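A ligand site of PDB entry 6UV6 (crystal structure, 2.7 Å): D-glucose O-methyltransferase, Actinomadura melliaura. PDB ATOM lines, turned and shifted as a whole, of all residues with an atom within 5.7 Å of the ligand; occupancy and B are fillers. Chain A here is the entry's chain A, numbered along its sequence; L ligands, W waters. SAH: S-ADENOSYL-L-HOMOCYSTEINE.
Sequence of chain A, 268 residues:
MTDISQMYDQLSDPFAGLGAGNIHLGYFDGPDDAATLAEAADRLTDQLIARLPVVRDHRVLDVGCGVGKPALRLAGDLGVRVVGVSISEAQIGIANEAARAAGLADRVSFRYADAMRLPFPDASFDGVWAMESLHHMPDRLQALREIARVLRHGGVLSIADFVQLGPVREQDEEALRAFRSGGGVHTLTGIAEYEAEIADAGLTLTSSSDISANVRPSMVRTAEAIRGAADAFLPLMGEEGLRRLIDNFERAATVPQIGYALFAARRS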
ATOM      1  N   TYR A   8      26.826 -27.679 -14.042  1.00  0.00           N
ATOM      2  CA  TYR A   8      25.722 -27.085 -14.786  1.00  0.00           C
ATOM      3  C   TYR A   8      26.099 -26.778 -16.227  1.00  0.00           C
ATOM      4  O   TYR A   8      25.389 -27.205 -17.157  1.00  0.00           O
ATOM      5  CB  TYR A   8      25.275 -25.837 -14.038  1.00  0.00           C
ATOM      6  CG  TYR A   8      24.200 -26.177 -13.031  1.00  0.00           C
ATOM      7  CD1 TYR A   8      22.867 -26.274 -13.413  1.00  0.00           C
ATOM      8  CD2 TYR A   8      24.533 -26.515 -11.734  1.00  0.00           C
ATOM      9  CE1 TYR A   8      21.886 -26.605 -12.510  1.00  0.00           C
ATOM     10  CE2 TYR A   8      23.557 -26.863 -10.816  1.00  0.00           C
ATOM     11  CZ  TYR A   8      22.242 -26.909 -11.209  1.00  0.00           C
ATOM     12  OH  TYR A   8      21.266 -27.264 -10.307  1.00  0.00           O
ATOM     13  N   GLY A  21      11.721 -26.437 -19.950  1.00  0.00           N
ATOM     14  CA  GLY A  21      12.749 -25.430 -19.754  1.00  0.00           C
ATOM     15  C   GLY A  21      13.067 -25.308 -18.280  1.00  0.00           C
ATOM     16  O   GLY A  21      13.829 -24.425 -17.860  1.00  0.00           O
ATOM     17  N   ASN A  22      12.493 -26.198 -17.482  1.00  0.00           N
ATOM     18  CA  ASN A  22      12.624 -26.182 -16.033  1.00  0.00           C
ATOM     19  C   ASN A  22      13.781 -27.062 -15.612  1.00  0.00           C
ATOM     20  O   ASN A  22      13.926 -28.197 -16.097  1.00  0.00           O
ATOM     21  CB  ASN A  22      11.325 -26.657 -15.371  1.00  0.00           C
ATOM     22  CG  ASN A  22      10.209 -25.645 -15.452  1.00  0.00           C
ATOM     23  OD1 ASN A  22      10.370 -24.493 -15.042  1.00  0.00           O
ATOM     24  ND2 ASN A  22       9.080 -26.062 -15.996  1.00  0.00           N
ATOM     25  N   ILE A  23      14.621 -26.546 -14.721  1.00  0.00           N
ATOM     26  CA  ILE A  23      15.687 -27.341 -14.131  1.00  0.00           C
ATOM     27  C   ILE A  23      15.398 -27.527 -12.656  1.00  0.00           C
ATOM     28  O   ILE A  23      16.174 -27.098 -11.795  1.00  0.00           O
ATOM     29  CB  ILE A  23      17.056 -26.676 -14.370  1.00  0.00           C
ATOM     30  CG1 ILE A  23      17.315 -26.550 -15.868  1.00  0.00           C
ATOM     31  CG2 ILE A  23      18.144 -27.508 -13.711  1.00  0.00           C
ATOM     32  CD1 ILE A  23      18.518 -25.715 -16.212  1.00  0.00           C
ATOM     33  N   HIS A  24      14.259 -28.137 -12.341  1.00  0.00           N
ATOM     34  CA  HIS A  24      13.890 -28.431 -10.970  1.00  0.00           C
ATOM     35  C   HIS A  24      12.901 -29.586 -10.986  1.00  0.00           C
ATOM     36  O   HIS A  24      12.421 -29.999 -12.038  1.00  0.00           O
ATOM     37  CB  HIS A  24      13.310 -27.197 -10.258  1.00  0.00           C
ATOM     38  CG  HIS A  24      12.056 -26.663 -10.869  1.00  0.00           C
ATOM     39  ND1 HIS A  24      12.037 -25.577 -11.713  1.00  0.00           N
ATOM     40  CD2 HIS A  24      10.766 -27.066 -10.746  1.00  0.00           C
ATOM     41  CE1 HIS A  24      10.791 -25.334 -12.096  1.00  0.00           C
ATOM     42  NE2 HIS A  24      10.006 -26.228 -11.519  1.00  0.00           N
ATOM     43  N   ASP A  62      15.434 -13.598  -9.148  1.00  0.00           N
ATOM     44  CA  ASP A  62      15.444 -15.048  -9.295  1.00  0.00           C
ATOM     45  C   ASP A  62      16.861 -15.531  -8.985  1.00  0.00           C
ATOM     46  O   ASP A  62      17.734 -15.518  -9.855  1.00  0.00           O
ATOM     47  CB  ASP A  62      15.003 -15.447 -10.698  1.00  0.00           C
ATOM     48  CG  ASP A  62      15.019 -16.951 -10.908  1.00  0.00           C
ATOM     49  OD1 ASP A  62      15.193 -17.700  -9.931  1.00  0.00           O
ATOM     50  OD2 ASP A  62      14.844 -17.392 -12.078  1.00  0.00           O
ATOM     51  N   VAL A  63      17.100 -15.949  -7.748  1.00  0.00           N
ATOM     52  CA  VAL A  63      18.403 -16.454  -7.342  1.00  0.00           C
ATOM     53  C   VAL A  63      18.546 -17.894  -7.841  1.00  0.00           C
ATOM     54  O   VAL A  63      17.799 -18.784  -7.439  1.00  0.00           O
ATOM     55  CB  VAL A  63      18.577 -16.395  -5.823  1.00  0.00           C
ATOM     56  CG1 VAL A  63      19.860 -17.084  -5.393  1.00  0.00           C
ATOM     57  CG2 VAL A  63      18.561 -14.947  -5.336  1.00  0.00           C
ATOM     58  N   GLY A  64      19.511 -18.111  -8.740  1.00  0.00           N
ATOM     59  CA  GLY A  64      19.639 -19.395  -9.403  1.00  0.00           C
ATOM     60  C   GLY A  64      18.551 -19.564 -10.449  1.00  0.00           C
ATOM     61  O   GLY A  64      17.613 -20.345 -10.263  1.00  0.00           O
ATOM     62  N   CYS A  65      18.694 -18.843 -11.562  1.00  0.00           N
ATOM     63  CA  CYS A  65      17.616 -18.691 -12.530  1.00  0.00           C
ATOM     64  C   CYS A  65      17.500 -19.845 -13.506  1.00  0.00           C
ATOM     65  O   CYS A  65      16.468 -19.963 -14.171  1.00  0.00           O
ATOM     66  CB  CYS A  65      17.824 -17.385 -13.294  1.00  0.00           C
ATOM     67  SG  CYS A  65      19.432 -17.295 -14.115  1.00  0.00           S
ATOM     68  N   GLY A  66      18.516 -20.687 -13.600  1.00  0.00           N
ATOM     69  CA  GLY A  66      18.497 -21.725 -14.622  1.00  0.00           C
ATOM     70  C   GLY A  66      18.520 -21.112 -16.001  1.00  0.00           C
ATOM     71  O   GLY A  66      19.259 -20.152 -16.271  1.00  0.00           O
ATOM     72  N   VAL A  67      17.689 -21.644 -16.891  1.00  0.00           N
ATOM     73  CA  VAL A  67      17.547 -21.094 -18.239  1.00  0.00           C
ATOM     74  C   VAL A  67      16.357 -20.154 -18.351  1.00  0.00           C
ATOM     75  O   VAL A  67      15.991 -19.749 -19.457  1.00  0.00           O
ATOM     76  CB  VAL A  67      17.475 -22.225 -19.288  1.00  0.00           C
ATOM     77  CG1 VAL A  67      18.797 -22.982 -19.330  1.00  0.00           C
ATOM     78  CG2 VAL A  67      16.306 -23.159 -19.005  1.00  0.00           C
ATOM     79  N   PRO A  70      11.118 -20.516 -15.138  1.00  0.00           N
ATOM     80  CA  PRO A  70      10.364 -20.029 -13.972  1.00  0.00           C
ATOM     81  C   PRO A  70      10.282 -18.514 -13.928  1.00  0.00           C
ATOM     82  O   PRO A  70       9.201 -17.963 -13.666  1.00  0.00           O
ATOM     83  CB  PRO A  70      11.153 -20.601 -12.793  1.00  0.00           C
ATOM     84  CG  PRO A  70      11.830 -21.815 -13.340  1.00  0.00           C
ATOM     85  CD  PRO A  70      12.191 -21.441 -14.755  1.00  0.00           C
ATOM     86  N   VAL A  85      19.746 -14.361 -11.647  1.00  0.00           N
ATOM     87  CA  VAL A  85      21.189 -14.469 -11.508  1.00  0.00           C
ATOM     88  C   VAL A  85      21.573 -15.932 -11.452  1.00  0.00           C
ATOM     89  O   VAL A  85      20.852 -16.778 -10.910  1.00  0.00           O
ATOM     90  CB  VAL A  85      21.726 -13.728 -10.266  1.00  0.00           C
ATOM     91  CG1 VAL A  85      21.422 -12.246 -10.354  1.00  0.00           C
ATOM     92  CG2 VAL A  85      21.122 -14.322  -8.995  1.00  0.00           C
ATOM     93  N   SER A  86      22.747 -16.218 -12.005  1.00  0.00           N
ATOM     94  CA  SER A  86      23.311 -17.556 -12.080  1.00  0.00           C
ATOM     95  C   SER A  86      24.823 -17.372 -12.123  1.00  0.00           C
ATOM     96  O   SER A  86      25.329 -16.257 -12.231  1.00  0.00           O
ATOM     97  CB  SER A  86      22.795 -18.311 -13.303  1.00  0.00           C
ATOM     98  OG  SER A  86      23.389 -19.586 -13.413  1.00  0.00           O
ATOM     99  N   ILE A  87      25.539 -18.481 -12.028  1.00  0.00           N
ATOM    100  CA  ILE A  87      26.987 -18.477 -12.180  1.00  0.00           C
ATOM    101  C   ILE A  87      27.419 -19.235 -13.425  1.00  0.00           C
ATOM    102  O   ILE A  87      28.607 -19.546 -13.574  1.00  0.00           O
ATOM    103  CB  ILE A  87      27.673 -19.038 -10.920  1.00  0.00           C
ATOM    104  CG1 ILE A  87      27.184 -20.456 -10.642  1.00  0.00           C
ATOM    105  CG2 ILE A  87      27.386 -18.138  -9.732  1.00  0.00           C
ATOM    106  CD1 ILE A  87      27.985 -21.177  -9.597  1.00  0.00           C
ATOM    107  N   SER A  88      26.491 -19.540 -14.311  1.00  0.00           N
ATOM    108  CA  SER A  88      26.763 -20.192 -15.585  1.00  0.00           C
ATOM    109  C   SER A  88      26.526 -19.194 -16.708  1.00  0.00           C
ATOM    110  O   SER A  88      25.379 -18.889 -17.053  1.00  0.00           O
ATOM    111  CB  SER A  88      25.897 -21.438 -15.752  1.00  0.00           C
ATOM    112  OG  SER A  88      25.934 -21.925 -17.087  1.00  0.00           O
ATOM    113  N   GLN A  91      24.159 -20.561 -19.247  1.00  0.00           N
ATOM    114  CA  GLN A  91      22.740 -20.510 -18.916  1.00  0.00           C
ATOM    115  C   GLN A  91      22.163 -19.115 -19.099  1.00  0.00           C
ATOM    116  O   GLN A  91      21.023 -18.947 -19.532  1.00  0.00           O
ATOM    117  CB  GLN A  91      22.513 -20.964 -17.484  1.00  0.00           C
ATOM    118  CG  GLN A  91      22.383 -22.455 -17.277  1.00  0.00           C
ATOM    119  CD  GLN A  91      22.138 -22.777 -15.812  1.00  0.00           C
ATOM    120  OE1 GLN A  91      22.013 -21.877 -14.984  1.00  0.00           O
ATOM    121  NE2 GLN A  91      22.071 -24.054 -15.493  1.00  0.00           N
ATOM    122  N   ALA A 113      25.988 -13.526 -11.415  1.00  0.00           N
ATOM    123  CA  ALA A 113      26.094 -13.112 -10.016  1.00  0.00           C
ATOM    124  C   ALA A 113      26.201 -14.359  -9.156  1.00  0.00           C
ATOM    125  O   ALA A 113      25.508 -15.346  -9.403  1.00  0.00           O
ATOM    126  CB  ALA A 113      24.888 -12.275  -9.586  1.00  0.00           C
ATOM    127  N   ASP A 114      27.065 -14.299  -8.155  1.00  0.00           N
ATOM    128  CA  ASP A 114      27.162 -15.335  -7.146  1.00  0.00           C
ATOM    129  C   ASP A 114      26.287 -14.887  -5.984  1.00  0.00           C
ATOM    130  O   ASP A 114      26.487 -13.797  -5.429  1.00  0.00           O
ATOM    131  CB  ASP A 114      28.612 -15.562  -6.715  1.00  0.00           C
ATOM    132  CG  ASP A 114      28.746 -16.618  -5.638  1.00  0.00           C
ATOM    133  OD1 ASP A 114      27.713 -17.178  -5.209  1.00  0.00           O
ATOM    134  OD2 ASP A 114      29.895 -16.897  -5.222  1.00  0.00           O
ATOM    135  N   ALA A 115      25.326 -15.738  -5.613  1.00  0.00           N
ATOM    136  CA  ALA A 115      24.328 -15.353  -4.623  1.00  0.00           C
ATOM    137  C   ALA A 115      24.930 -14.970  -3.284  1.00  0.00           C
ATOM    138  O   ALA A 115      24.223 -14.389  -2.449  1.00  0.00           O
ATOM    139  CB  ALA A 115      23.337 -16.502  -4.430  1.00  0.00           C
ATOM    140  N   MET A 116      26.205 -15.267  -3.048  1.00  0.00           N
ATOM    141  CA  MET A 116      26.835 -14.959  -1.769  1.00  0.00           C
ATOM    142  C   MET A 116      27.404 -13.554  -1.718  1.00  0.00           C
ATOM    143  O   MET A 116      27.742 -13.082  -0.628  1.00  0.00           O
ATOM    144  CB  MET A 116      27.918 -15.991  -1.463  1.00  0.00           C
ATOM    145  CG  MET A 116      27.331 -17.353  -1.112  1.00  0.00           C
ATOM    146  SD  MET A 116      28.492 -18.543  -0.421  1.00  0.00           S
ATOM    147  CE  MET A 116      29.622 -18.825  -1.783  1.00  0.00           C
ATOM    148  N   TRP A 129      13.128 -14.946  -5.169  1.00  0.00           N
ATOM    149  CA  TRP A 129      12.601 -16.224  -5.631  1.00  0.00           C
ATOM    150  C   TRP A 129      13.769 -17.174  -5.802  1.00  0.00           C
ATOM    151  O   TRP A 129      14.617 -16.982  -6.688  1.00  0.00           O
ATOM    152  CB  TRP A 129      11.830 -16.033  -6.953  1.00  0.00           C
ATOM    153  CG  TRP A 129      11.577 -17.258  -7.771  1.00  0.00           C
ATOM    154  CD1 TRP A 129      12.466 -17.879  -8.607  1.00  0.00           C
ATOM    155  CD2 TRP A 129      10.348 -17.983  -7.884  1.00  0.00           C
ATOM    156  NE1 TRP A 129      11.865 -18.961  -9.210  1.00  0.00           N
ATOM    157  CE2 TRP A 129      10.567 -19.047  -8.784  1.00  0.00           C
ATOM    158  CE3 TRP A 129       9.086 -17.835  -7.300  1.00  0.00           C
ATOM    159  CZ2 TRP A 129       9.564 -19.954  -9.117  1.00  0.00           C
ATOM    160  CZ3 TRP A 129       8.096 -18.748  -7.630  1.00  0.00           C
ATOM    161  CH2 TRP A 129       8.347 -19.793  -8.525  1.00  0.00           C
ATOM    162  N   MET A 131      14.190 -20.959  -6.308  1.00  0.00           N
ATOM    163  CA  MET A 131      13.640 -22.286  -6.575  1.00  0.00           C
ATOM    164  C   MET A 131      14.785 -23.287  -6.685  1.00  0.00           C
ATOM    165  O   MET A 131      15.536 -23.273  -7.674  1.00  0.00           O
ATOM    166  CB  MET A 131      12.792 -22.312  -7.835  1.00  0.00           C
ATOM    167  CG  MET A 131      12.381 -23.729  -8.188  1.00  0.00           C
ATOM    168  SD  MET A 131      10.776 -23.806  -8.979  1.00  0.00           S
ATOM    169  CE  MET A 131       9.681 -23.862  -7.557  1.00  0.00           C
ATOM    170  N   GLU A 132      14.920 -24.159  -5.683  1.00  0.00           N
ATOM    171  CA  GLU A 132      15.802 -25.314  -5.766  1.00  0.00           C
ATOM    172  C   GLU A 132      17.225 -24.908  -6.123  1.00  0.00           C
ATOM    173  O   GLU A 132      17.867 -25.497  -7.001  1.00  0.00           O
ATOM    174  CB  GLU A 132      15.263 -26.332  -6.781  1.00  0.00           C
ATOM    175  CG  GLU A 132      15.703 -27.758  -6.555  1.00  0.00           C
ATOM    176  CD  GLU A 132      14.859 -28.754  -7.333  1.00  0.00           C
ATOM    177  OE1 GLU A 132      13.623 -28.769  -7.125  1.00  0.00           O
ATOM    178  OE2 GLU A 132      15.426 -29.504  -8.149  1.00  0.00           O
ATOM    179  N   SER A 133      17.729 -23.890  -5.416  1.00  0.00           N
ATOM    180  CA  SER A 133      19.044 -23.363  -5.725  1.00  0.00           C
ATOM    181  C   SER A 133      19.917 -23.176  -4.490  1.00  0.00           C
ATOM    182  O   SER A 133      21.149 -23.276  -4.579  1.00  0.00           O
ATOM    183  CB  SER A 133      18.907 -22.032  -6.472  1.00  0.00           C
ATOM    184  OG  SER A 133      18.301 -21.061  -5.635  1.00  0.00           O
ATOM    185  N   HIS A 136      22.975 -25.370  -3.278  1.00  0.00           N
ATOM    186  CA  HIS A 136      24.271 -25.281  -3.942  1.00  0.00           C
ATOM    187  C   HIS A 136      25.228 -24.318  -3.259  1.00  0.00           C
ATOM    188  O   HIS A 136      26.361 -24.171  -3.706  1.00  0.00           O
ATOM    189  CB  HIS A 136      24.103 -24.835  -5.407  1.00  0.00           C
ATOM    190  CG  HIS A 136      23.260 -25.752  -6.235  1.00  0.00           C
ATOM    191  ND1 HIS A 136      23.595 -27.068  -6.475  1.00  0.00           N
ATOM    192  CD2 HIS A 136      22.102 -25.541  -6.907  1.00  0.00           C
ATOM    193  CE1 HIS A 136      22.678 -27.629  -7.239  1.00  0.00           C
ATOM    194  NE2 HIS A 136      21.764 -26.717  -7.515  1.00  0.00           N
ATOM    195  N   MET A 137      24.789 -23.644  -2.205  1.00  0.00           N
ATOM    196  CA  MET A 137      25.579 -22.626  -1.522  1.00  0.00           C
ATOM    197  C   MET A 137      26.483 -23.259  -0.465  1.00  0.00           C
ATOM    198  O   MET A 137      26.001 -24.038   0.360  1.00  0.00           O
ATOM    199  CB  MET A 137      24.665 -21.595  -0.876  1.00  0.00           C
ATOM    200  CG  MET A 137      23.637 -21.016  -1.822  1.00  0.00           C
ATOM    201  SD  MET A 137      24.380 -20.138  -3.217  1.00  0.00           S
ATOM    202  CE  MET A 137      22.954 -19.984  -4.298  1.00  0.00           C
ATOM    203  N   PRO A 138      27.784 -22.936  -0.459  1.00  0.00           N
ATOM    204  CA  PRO A 138      28.615 -23.420   0.653  1.00  0.00           C
ATOM    205  C   PRO A 138      28.229 -22.791   1.986  1.00  0.00           C
ATOM    206  O   PRO A 138      28.241 -23.486   3.009  1.00  0.00           O
ATOM    207  CB  PRO A 138      30.042 -23.002   0.239  1.00  0.00           C
ATOM    208  CG  PRO A 138      29.965 -22.696  -1.214  1.00  0.00           C
ATOM    209  CD  PRO A 138      28.570 -22.259  -1.508  1.00  0.00           C
HETATM  210  N   SAH L   1      15.550 -21.592 -10.983  1.00  0.00           N
HETATM  211  CA  SAH L   1      15.812 -22.518 -12.025  1.00  0.00           C
HETATM  212  CB  SAH L   1      17.217 -23.164 -11.843  1.00  0.00           C
HETATM  213  CG  SAH L   1      17.408 -23.971 -10.563  1.00  0.00           C
HETATM  214  SD  SAH L   1      18.913 -24.933 -10.886  1.00  0.00           S
HETATM  215  C   SAH L   1      14.747 -23.604 -12.153  1.00  0.00           C
HETATM  216  O   SAH L   1      14.127 -24.067 -11.214  1.00  0.00           O
HETATM  217  OXT SAH L   1      14.588 -23.971 -13.383  1.00  0.00           O
HETATM  218  C5' SAH L   1      20.146 -24.197  -9.780  1.00  0.00           C
HETATM  219  C4' SAH L   1      20.617 -22.862 -10.326  1.00  0.00           C
HETATM  220  O4' SAH L   1      21.362 -22.159  -9.315  1.00  0.00           O
HETATM  221  C3' SAH L   1      21.529 -22.955 -11.554  1.00  0.00           C
HETATM  222  O3' SAH L   1      21.161 -21.964 -12.517  1.00  0.00           O
HETATM  223  C2' SAH L   1      22.917 -22.651 -10.974  1.00  0.00           C
HETATM  224  O2' SAH L   1      23.796 -22.060 -11.915  1.00  0.00           O
HETATM  225  C1' SAH L   1      22.540 -21.643  -9.898  1.00  0.00           C
HETATM  226  N9  SAH L   1      23.549 -21.428  -8.864  1.00  0.00           N
HETATM  227  C8  SAH L   1      24.326 -22.367  -8.253  1.00  0.00           C
HETATM  228  N7  SAH L   1      25.176 -21.873  -7.376  1.00  0.00           N
HETATM  229  C5  SAH L   1      24.918 -20.508  -7.420  1.00  0.00           C
HETATM  230  C6  SAH L   1      25.481 -19.423  -6.725  1.00  0.00           C
HETATM  231  N6  SAH L   1      26.460 -19.543  -5.814  1.00  0.00           N
HETATM  232  N1  SAH L   1      25.002 -18.191  -6.993  1.00  0.00           N
HETATM  233  C2  SAH L   1      24.026 -18.062  -7.902  1.00  0.00           C
HETATM  234  N3  SAH L   1      23.425 -19.017  -8.616  1.00  0.00           N
HETATM  235  C4  SAH L   1      23.919 -20.225  -8.333  1.00  0.00           C
HETATM  236  O   HOH W   1      15.267 -22.979 -16.191  1.00  0.00           O
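An oxygen (OXT) of the ligand is in hydrogen-bond range of the backbone NH (N) of Ile 23, 2.9 Å away. The side-chain hydroxyl (OH) of Tyr 8 sits close to a sulfur (SD) of the ligand. OG of Ser 86 lies within hydrogen-bond range of O2' of the ligand (2.9 Å). O of Gly 64 lies within hydrogen-bond range of N of the ligand (2.5 Å). A ring nitrogen (ND1) of His 24 lies within hydrogen-bond range of an oxygen (O) of the ligand (2.6 Å). The side-chain amide oxygen of Gln 91 lies within hydrogen-bond range of an oxygen (O3') of the ligand, 2.6 Å away. The side-chain carboxylate (OD1) of Asp 114 lies within hydrogen-bond range of a nitrogen (N6) of the ligand (2.7 Å). A nitrogen (N6) of the ligand sits at hydrogen-bond distance from the side-chain sulfur (SD) of Met 137 (3.4 Å). The backbone NH (N) of Ala 115 is in hydrogen-bond range of a nitrogen (N1) of the ligand (2.8 Å). The backbone NH (N) of Gly 66 lies within hydrogen-bond range of an oxygen (O3') of the ligand, 3.1 Å away.
The backbone NH (N) of Gln 91 sits at hydrogen-bond distance from the side-chain hydroxyl (OG) of Ser 88 (3.1 Å). OE1 of Gln 91 sits at hydrogen-bond distance from OG of Ser 86 (3.1 Å). The backbone carbonyl oxygen (O) of Val 63 is in hydrogen-bond range of the side-chain hydroxyl (OG) of Ser 133, 2.9 Å away. N of Cys 65 is in hydrogen-bond range of O of Val 85 (3.1 Å). The backbone carbonyl oxygen (O) of Ser 86 lies within hydrogen-bond range of the backbone NH (N) of Ala 113, 2.9 Å away. The side-chain amide oxygen (OE1) of Gln 91 sits close to the backbone carbonyl oxygen (O) of Gly 66. N of Met 116 sits close to OD1 of Asp 114, 3.3 Å away. A ring nitrogen (ND1) of His 24 sits close to the side-chain sulfur of Met 131 (3.5 Å).
C of Asn 22 touches OXT of the ligand, at 3.9 Å. Cys 65 touches the ligand (O to CA, 3.4 Å). CG of Pro 70 touches OXT of the ligand (3.5 Å). Ile 87 touches the ligand. Ala 113 touches the ligand. Met 131 touches the ligand. O of Glu 132 touches C5' of the ligand (3.8 Å). Ser 133 touches the ligand. His 136 touches the ligand. Hydrophobic or aromatic side chains that line the ligand: Tyr 8, Ile 23, His 24, Pro 70, Ile 87, Ala 115, Met 131, His 136 and Met 137. Within 4 Å of the ligand: Tyr 8, Asn 22, Ile 23, His 24, Gly 64, Cys 65, Gly 66, Pro 70, Ser 86, Ile 87, Gln 91, Ala 113, Asp 114, Ala 115, Met 131, Glu 132, Ser 133, His 136 and Met 137.
Water W1 lies within hydrogen-bond range of the backbone carbonyl oxygen (O) of Gly 21 (2.6 Å), the backbone NH (N) of Val 67 (2.9 Å) and an oxygen (OXT) of the ligand (3.1 Å).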
